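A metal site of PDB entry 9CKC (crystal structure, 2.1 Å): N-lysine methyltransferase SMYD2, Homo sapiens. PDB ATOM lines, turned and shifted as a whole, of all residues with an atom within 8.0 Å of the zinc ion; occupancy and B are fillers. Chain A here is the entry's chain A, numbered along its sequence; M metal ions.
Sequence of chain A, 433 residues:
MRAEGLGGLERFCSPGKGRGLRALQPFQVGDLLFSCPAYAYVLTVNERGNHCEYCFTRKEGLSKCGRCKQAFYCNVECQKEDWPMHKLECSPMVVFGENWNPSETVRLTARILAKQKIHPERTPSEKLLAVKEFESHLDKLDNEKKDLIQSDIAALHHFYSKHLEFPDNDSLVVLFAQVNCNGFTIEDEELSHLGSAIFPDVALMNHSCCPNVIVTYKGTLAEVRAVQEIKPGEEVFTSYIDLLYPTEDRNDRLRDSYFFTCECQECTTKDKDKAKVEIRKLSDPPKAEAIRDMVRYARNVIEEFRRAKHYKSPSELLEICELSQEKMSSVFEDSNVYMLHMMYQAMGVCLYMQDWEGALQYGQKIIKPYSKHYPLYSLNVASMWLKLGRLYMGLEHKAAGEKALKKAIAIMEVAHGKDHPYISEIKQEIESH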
ATOM      1  N   LYS A  64     -13.574 -25.206  21.624  1.00  0.00           N
ATOM      2  CA  LYS A  64     -13.283 -25.629  20.260  1.00  0.00           C
ATOM      3  C   LYS A  64     -14.560 -26.012  19.525  1.00  0.00           C
ATOM      4  O   LYS A  64     -15.434 -26.677  20.085  1.00  0.00           O
ATOM      5  CB  LYS A  64     -12.295 -26.800  20.279  1.00  0.00           C
ATOM      6  CG  LYS A  64     -11.927 -27.343  18.915  1.00  0.00           C
ATOM      7  CD  LYS A  64     -10.711 -28.256  19.016  1.00  0.00           C
ATOM      8  CE  LYS A  64     -11.003 -29.474  19.866  1.00  0.00           C
ATOM      9  NZ  LYS A  64      -9.800 -30.356  20.019  1.00  0.00           N
ATOM     10  N   CYS A  65     -14.672 -25.570  18.270  1.00  0.00           N
ATOM     11  CA  CYS A  65     -15.838 -25.907  17.455  1.00  0.00           C
ATOM     12  C   CYS A  65     -15.889 -27.415  17.209  1.00  0.00           C
ATOM     13  O   CYS A  65     -14.969 -27.985  16.624  1.00  0.00           O
ATOM     14  CB  CYS A  65     -15.785 -25.158  16.120  1.00  0.00           C
ATOM     15  SG  CYS A  65     -17.179 -25.523  15.011  1.00  0.00           S
ATOM     16  N   GLY A  66     -16.965 -28.049  17.669  1.00  0.00           N
ATOM     17  CA  GLY A  66     -17.075 -29.500  17.604  1.00  0.00           C
ATOM     18  C   GLY A  66     -17.115 -30.067  16.200  1.00  0.00           C
ATOM     19  O   GLY A  66     -16.840 -31.257  16.023  1.00  0.00           O
ATOM     20  N   ARG A  67     -17.468 -29.256  15.204  1.00  0.00           N
ATOM     21  CA  ARG A  67     -17.613 -29.764  13.844  1.00  0.00           C
ATOM     22  C   ARG A  67     -16.257 -29.849  13.134  1.00  0.00           C
ATOM     23  O   ARG A  67     -15.864 -30.911  12.640  1.00  0.00           O
ATOM     24  CB  ARG A  67     -18.576 -28.884  13.061  1.00  0.00           C
ATOM     25  CG  ARG A  67     -19.918 -28.742  13.742  1.00  0.00           C
ATOM     26  CD  ARG A  67     -20.851 -27.792  13.009  1.00  0.00           C
ATOM     27  NE  ARG A  67     -21.924 -27.343  13.889  1.00  0.00           N
ATOM     28  CZ  ARG A  67     -22.936 -26.568  13.501  1.00  0.00           C
ATOM     29  NH1 ARG A  67     -23.025 -26.193  12.241  1.00  0.00           N
ATOM     30  NH2 ARG A  67     -23.863 -26.192  14.368  1.00  0.00           N
ATOM     31  N   CYS A  68     -15.564 -28.718  13.061  1.00  0.00           N
ATOM     32  CA  CYS A  68     -14.310 -28.608  12.332  1.00  0.00           C
ATOM     33  C   CYS A  68     -13.074 -28.679  13.234  1.00  0.00           C
ATOM     34  O   CYS A  68     -11.974 -28.935  12.724  1.00  0.00           O
ATOM     35  CB  CYS A  68     -14.291 -27.311  11.524  1.00  0.00           C
ATOM     36  SG  CYS A  68     -14.265 -25.801  12.533  1.00  0.00           S
ATOM     37  N   LYS A  69     -13.238 -28.449  14.544  1.00  0.00           N
ATOM     38  CA  LYS A  69     -12.132 -28.502  15.507  1.00  0.00           C
ATOM     39  C   LYS A  69     -10.987 -27.565  15.119  1.00  0.00           C
ATOM     40  O   LYS A  69      -9.831 -27.812  15.461  1.00  0.00           O
ATOM     41  CB  LYS A  69     -11.615 -29.933  15.678  1.00  0.00           C
ATOM     42  CG  LYS A  69     -12.508 -30.841  16.503  1.00  0.00           C
ATOM     43  CD  LYS A  69     -13.441 -31.661  15.640  1.00  0.00           C
ATOM     44  CE  LYS A  69     -14.082 -32.784  16.447  1.00  0.00           C
ATOM     45  NZ  LYS A  69     -15.081 -33.538  15.646  1.00  0.00           N
ATOM     46  N   GLN A  70     -11.306 -26.477  14.418  1.00  0.00           N
ATOM     47  CA  GLN A  70     -10.254 -25.583  13.963  1.00  0.00           C
ATOM     48  C   GLN A  70     -10.625 -24.106  14.153  1.00  0.00           C
ATOM     49  O   GLN A  70     -10.027 -23.233  13.522  1.00  0.00           O
ATOM     50  CB  GLN A  70      -9.911 -25.873  12.508  1.00  0.00           C
ATOM     51  CG  GLN A  70      -9.085 -27.136  12.333  1.00  0.00           C
ATOM     52  CD  GLN A  70      -8.742 -27.415  10.887  1.00  0.00           C
ATOM     53  OE1 GLN A  70      -7.664 -27.062  10.412  1.00  0.00           O
ATOM     54  NE2 GLN A  70      -9.658 -28.075  10.177  1.00  0.00           N
ATOM     55  N   ALA A  71     -11.603 -23.827  15.005  1.00  0.00           N
ATOM     56  CA  ALA A  71     -11.992 -22.471  15.379  1.00  0.00           C
ATOM     57  C   ALA A  71     -12.317 -22.484  16.861  1.00  0.00           C
ATOM     58  O   ALA A  71     -13.085 -23.330  17.328  1.00  0.00           O
ATOM     59  CB  ALA A  71     -13.196 -21.981  14.558  1.00  0.00           C
ATOM     60  N   PHE A  72     -11.711 -21.555  17.607  1.00  0.00           N
ATOM     61  CA  PHE A  72     -11.834 -21.534  19.056  1.00  0.00           C
ATOM     62  C   PHE A  72     -12.538 -20.264  19.501  1.00  0.00           C
ATOM     63  O   PHE A  72     -12.456 -19.231  18.838  1.00  0.00           O
ATOM     64  CB  PHE A  72     -10.450 -21.664  19.716  1.00  0.00           C
ATOM     65  CG  PHE A  72      -9.765 -22.971  19.436  1.00  0.00           C
ATOM     66  CD1 PHE A  72      -9.175 -23.220  18.201  1.00  0.00           C
ATOM     67  CD2 PHE A  72      -9.712 -23.968  20.401  1.00  0.00           C
ATOM     68  CE1 PHE A  72      -8.546 -24.418  17.938  1.00  0.00           C
ATOM     69  CE2 PHE A  72      -9.079 -25.174  20.139  1.00  0.00           C
ATOM     70  CZ  PHE A  72      -8.496 -25.394  18.911  1.00  0.00           C
ATOM     71  N   TYR A  73     -13.248 -20.352  20.624  1.00  0.00           N
ATOM     72  CA  TYR A  73     -14.130 -19.282  21.076  1.00  0.00           C
ATOM     73  C   TYR A  73     -14.069 -19.129  22.585  1.00  0.00           C
ATOM     74  O   TYR A  73     -13.756 -20.076  23.312  1.00  0.00           O
ATOM     75  CB  TYR A  73     -15.586 -19.558  20.659  1.00  0.00           C
ATOM     76  CG  TYR A  73     -15.772 -19.597  19.167  1.00  0.00           C
ATOM     77  CD1 TYR A  73     -15.795 -18.429  18.423  1.00  0.00           C
ATOM     78  CD2 TYR A  73     -15.927 -20.805  18.492  1.00  0.00           C
ATOM     79  CE1 TYR A  73     -15.966 -18.451  17.062  1.00  0.00           C
ATOM     80  CE2 TYR A  73     -16.095 -20.848  17.124  1.00  0.00           C
ATOM     81  CZ  TYR A  73     -16.120 -19.668  16.411  1.00  0.00           C
ATOM     82  OH  TYR A  73     -16.283 -19.686  15.047  1.00  0.00           O
ATOM     83  N   GLN A  79     -19.229 -18.028  19.950  1.00  0.00           N
ATOM     84  CA  GLN A  79     -19.375 -19.027  18.903  1.00  0.00           C
ATOM     85  C   GLN A  79     -20.622 -18.772  18.051  1.00  0.00           C
ATOM     86  O   GLN A  79     -20.568 -18.856  16.822  1.00  0.00           O
ATOM     87  CB  GLN A  79     -19.425 -20.429  19.518  1.00  0.00           C
ATOM     88  CG  GLN A  79     -19.574 -21.554  18.521  1.00  0.00           C
ATOM     89  CD  GLN A  79     -19.433 -22.898  19.177  1.00  0.00           C
ATOM     90  OE1 GLN A  79     -19.308 -23.004  20.398  1.00  0.00           O
ATOM     91  NE2 GLN A  79     -19.481 -23.957  18.369  1.00  0.00           N
ATOM     92  N   ASP A  82     -20.290 -15.649  15.820  1.00  0.00           N
ATOM     93  CA  ASP A  82     -19.370 -15.844  14.711  1.00  0.00           C
ATOM     94  C   ASP A  82     -19.905 -16.784  13.631  1.00  0.00           C
ATOM     95  O   ASP A  82     -19.319 -16.850  12.542  1.00  0.00           O
ATOM     96  CB  ASP A  82     -18.026 -16.380  15.225  1.00  0.00           C
ATOM     97  CG  ASP A  82     -16.934 -16.274  14.185  1.00  0.00           C
ATOM     98  OD1 ASP A  82     -16.790 -15.191  13.576  1.00  0.00           O
ATOM     99  OD2 ASP A  82     -16.201 -17.275  13.984  1.00  0.00           O
ATOM    100  N   TRP A  83     -20.978 -17.528  13.920  1.00  0.00           N
ATOM    101  CA  TRP A  83     -21.502 -18.516  12.988  1.00  0.00           C
ATOM    102  C   TRP A  83     -21.799 -17.988  11.582  1.00  0.00           C
ATOM    103  O   TRP A  83     -21.433 -18.669  10.615  1.00  0.00           O
ATOM    104  CB  TRP A  83     -22.750 -19.186  13.579  1.00  0.00           C
ATOM    105  CG  TRP A  83     -23.285 -20.270  12.703  1.00  0.00           C
ATOM    106  CD1 TRP A  83     -24.525 -20.313  12.130  1.00  0.00           C
ATOM    107  CD2 TRP A  83     -22.578 -21.413  12.208  1.00  0.00           C
ATOM    108  NE1 TRP A  83     -24.649 -21.442  11.352  1.00  0.00           N
ATOM    109  CE2 TRP A  83     -23.462 -22.135  11.382  1.00  0.00           C
ATOM    110  CE3 TRP A  83     -21.284 -21.920  12.409  1.00  0.00           C
ATOM    111  CZ2 TRP A  83     -23.100 -23.329  10.755  1.00  0.00           C
ATOM    112  CZ3 TRP A  83     -20.926 -23.105  11.782  1.00  0.00           C
ATOM    113  CH2 TRP A  83     -21.834 -23.781  10.965  1.00  0.00           C
ATOM    114  N   HIS A  86     -18.314 -17.928  10.163  1.00  0.00           N
ATOM    115  CA  HIS A  86     -17.569 -19.178  10.270  1.00  0.00           C
ATOM    116  C   HIS A  86     -18.109 -20.258   9.331  1.00  0.00           C
ATOM    117  O   HIS A  86     -17.331 -21.091   8.862  1.00  0.00           O
ATOM    118  CB  HIS A  86     -17.603 -19.661  11.714  1.00  0.00           C
ATOM    119  CG  HIS A  86     -16.876 -20.952  11.934  1.00  0.00           C
ATOM    120  ND1 HIS A  86     -15.574 -21.152  11.516  1.00  0.00           N
ATOM    121  CD2 HIS A  86     -17.273 -22.106  12.504  1.00  0.00           C
ATOM    122  CE1 HIS A  86     -15.208 -22.384  11.823  1.00  0.00           C
ATOM    123  NE2 HIS A  86     -16.213 -22.977  12.433  1.00  0.00           N
ATOM    124  N   LYS A  87     -19.415 -20.269   9.064  1.00  0.00           N
ATOM    125  CA  LYS A  87     -19.988 -21.312   8.214  1.00  0.00           C
ATOM    126  C   LYS A  87     -19.469 -21.251   6.775  1.00  0.00           C
ATOM    127  O   LYS A  87     -19.678 -22.197   6.006  1.00  0.00           O
ATOM    128  CB  LYS A  87     -21.516 -21.247   8.221  1.00  0.00           C
ATOM    129  CG  LYS A  87     -22.149 -20.030   7.587  1.00  0.00           C
ATOM    130  CD  LYS A  87     -23.668 -20.171   7.657  1.00  0.00           C
ATOM    131  CE  LYS A  87     -24.398 -18.978   7.072  1.00  0.00           C
ATOM    132  NZ  LYS A  87     -25.875 -19.130   7.206  1.00  0.00           N
ATOM    133  N   GLU A  89     -16.421 -21.440   6.118  1.00  0.00           N
ATOM    134  CA  GLU A  89     -15.206 -22.241   6.152  1.00  0.00           C
ATOM    135  C   GLU A  89     -15.331 -23.515   6.969  1.00  0.00           C
ATOM    136  O   GLU A  89     -14.535 -24.438   6.740  1.00  0.00           O
ATOM    137  CB  GLU A  89     -14.046 -21.410   6.720  1.00  0.00           C
ATOM    138  CG  GLU A  89     -13.758 -20.157   5.917  1.00  0.00           C
ATOM    139  CD  GLU A  89     -12.639 -19.310   6.485  1.00  0.00           C
ATOM    140  OE1 GLU A  89     -12.414 -19.364   7.715  1.00  0.00           O
ATOM    141  OE2 GLU A  89     -11.979 -18.599   5.696  1.00  0.00           O
ATOM    142  N   CYS A  90     -16.271 -23.591   7.908  1.00  0.00           N
ATOM    143  CA  CYS A  90     -16.349 -24.707   8.837  1.00  0.00           C
ATOM    144  C   CYS A  90     -16.334 -26.048   8.101  1.00  0.00           C
ATOM    145  O   CYS A  90     -15.383 -26.837   8.221  1.00  0.00           O
ATOM    146  CB  CYS A  90     -17.607 -24.580   9.709  1.00  0.00           C
ATOM    147  SG  CYS A  90     -17.709 -25.813  11.027  1.00  0.00           S
ATOM    148  N   SER A  91     -17.388 -26.325   7.332  1.00  0.00           N
ATOM    149  CA  SER A  91     -17.445 -27.585   6.603  1.00  0.00           C
ATOM    150  C   SER A  91     -16.383 -27.691   5.501  1.00  0.00           C
ATOM    151  O   SER A  91     -15.726 -28.733   5.410  1.00  0.00           O
ATOM    152  CB  SER A  91     -18.851 -27.810   6.050  1.00  0.00           C
ATOM    153  OG  SER A  91     -18.943 -29.076   5.421  1.00  0.00           O
ATOM    154  N   MET A  93     -13.404 -26.662   5.400  1.00  0.00           N
ATOM    155  CA  MET A  93     -12.106 -26.983   5.990  1.00  0.00           C
ATOM    156  C   MET A  93     -11.951 -28.489   6.214  1.00  0.00           C
ATOM    157  O   MET A  93     -10.871 -29.043   5.970  1.00  0.00           O
ATOM    158  CB  MET A  93     -11.918 -26.236   7.305  1.00  0.00           C
ATOM    159  CG  MET A  93     -11.453 -24.804   7.136  1.00  0.00           C
ATOM    160  SD  MET A  93     -10.759 -24.121   8.649  1.00  0.00           S
ATOM    161  CE  MET A  93     -12.209 -24.023   9.690  1.00  0.00           C
ATOM    162  N   VAL A  94     -13.000 -29.154   6.682  1.00  0.00           N
ATOM    163  CA  VAL A  94     -12.904 -30.597   6.901  1.00  0.00           C
ATOM    164  C   VAL A  94     -12.985 -31.356   5.585  1.00  0.00           C
ATOM    165  O   VAL A  94     -12.270 -32.333   5.363  1.00  0.00           O
ATOM    166  CB  VAL A  94     -13.994 -31.075   7.870  1.00  0.00           C
ATOM    167  CG1 VAL A  94     -13.634 -32.438   8.435  1.00  0.00           C
ATOM    168  CG2 VAL A  94     -14.197 -30.067   8.991  1.00  0.00           C
HETATM  169 ZN    ZN M   1     -16.403 -25.020  12.762  1.00  0.00          ZN
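The zinc ion is bound by a ring nitrogen (NE2) of His 86 (2.1 Å), the side-chain sulfur (SG) of Cys 68 (2.3 Å), the side-chain sulfur (SG) of Cys 90 (2.3 Å) and the side-chain sulfur (SG) of Cys 65 (2.4 Å).
The zinc ion has four donor atoms within binding distance.
Of the 20 residues printed, 4 come within 4 Å of the zinc ion.
The nearest printed residue that does not touch the zinc ion is Arg 67 (4.4 Å).
SG of Cys 68 sits close to N of Gln 70 (3.6 Å).
The backbone NH of Arg 67 lies close to the side-chain sulfur of Cys 65, at 3.7 Å.
The backbone carbonyl oxygen (O) of Ala 71 is in hydrogen-bond range of the backbone NH (N) of Cys 65, at 2.9 Å.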
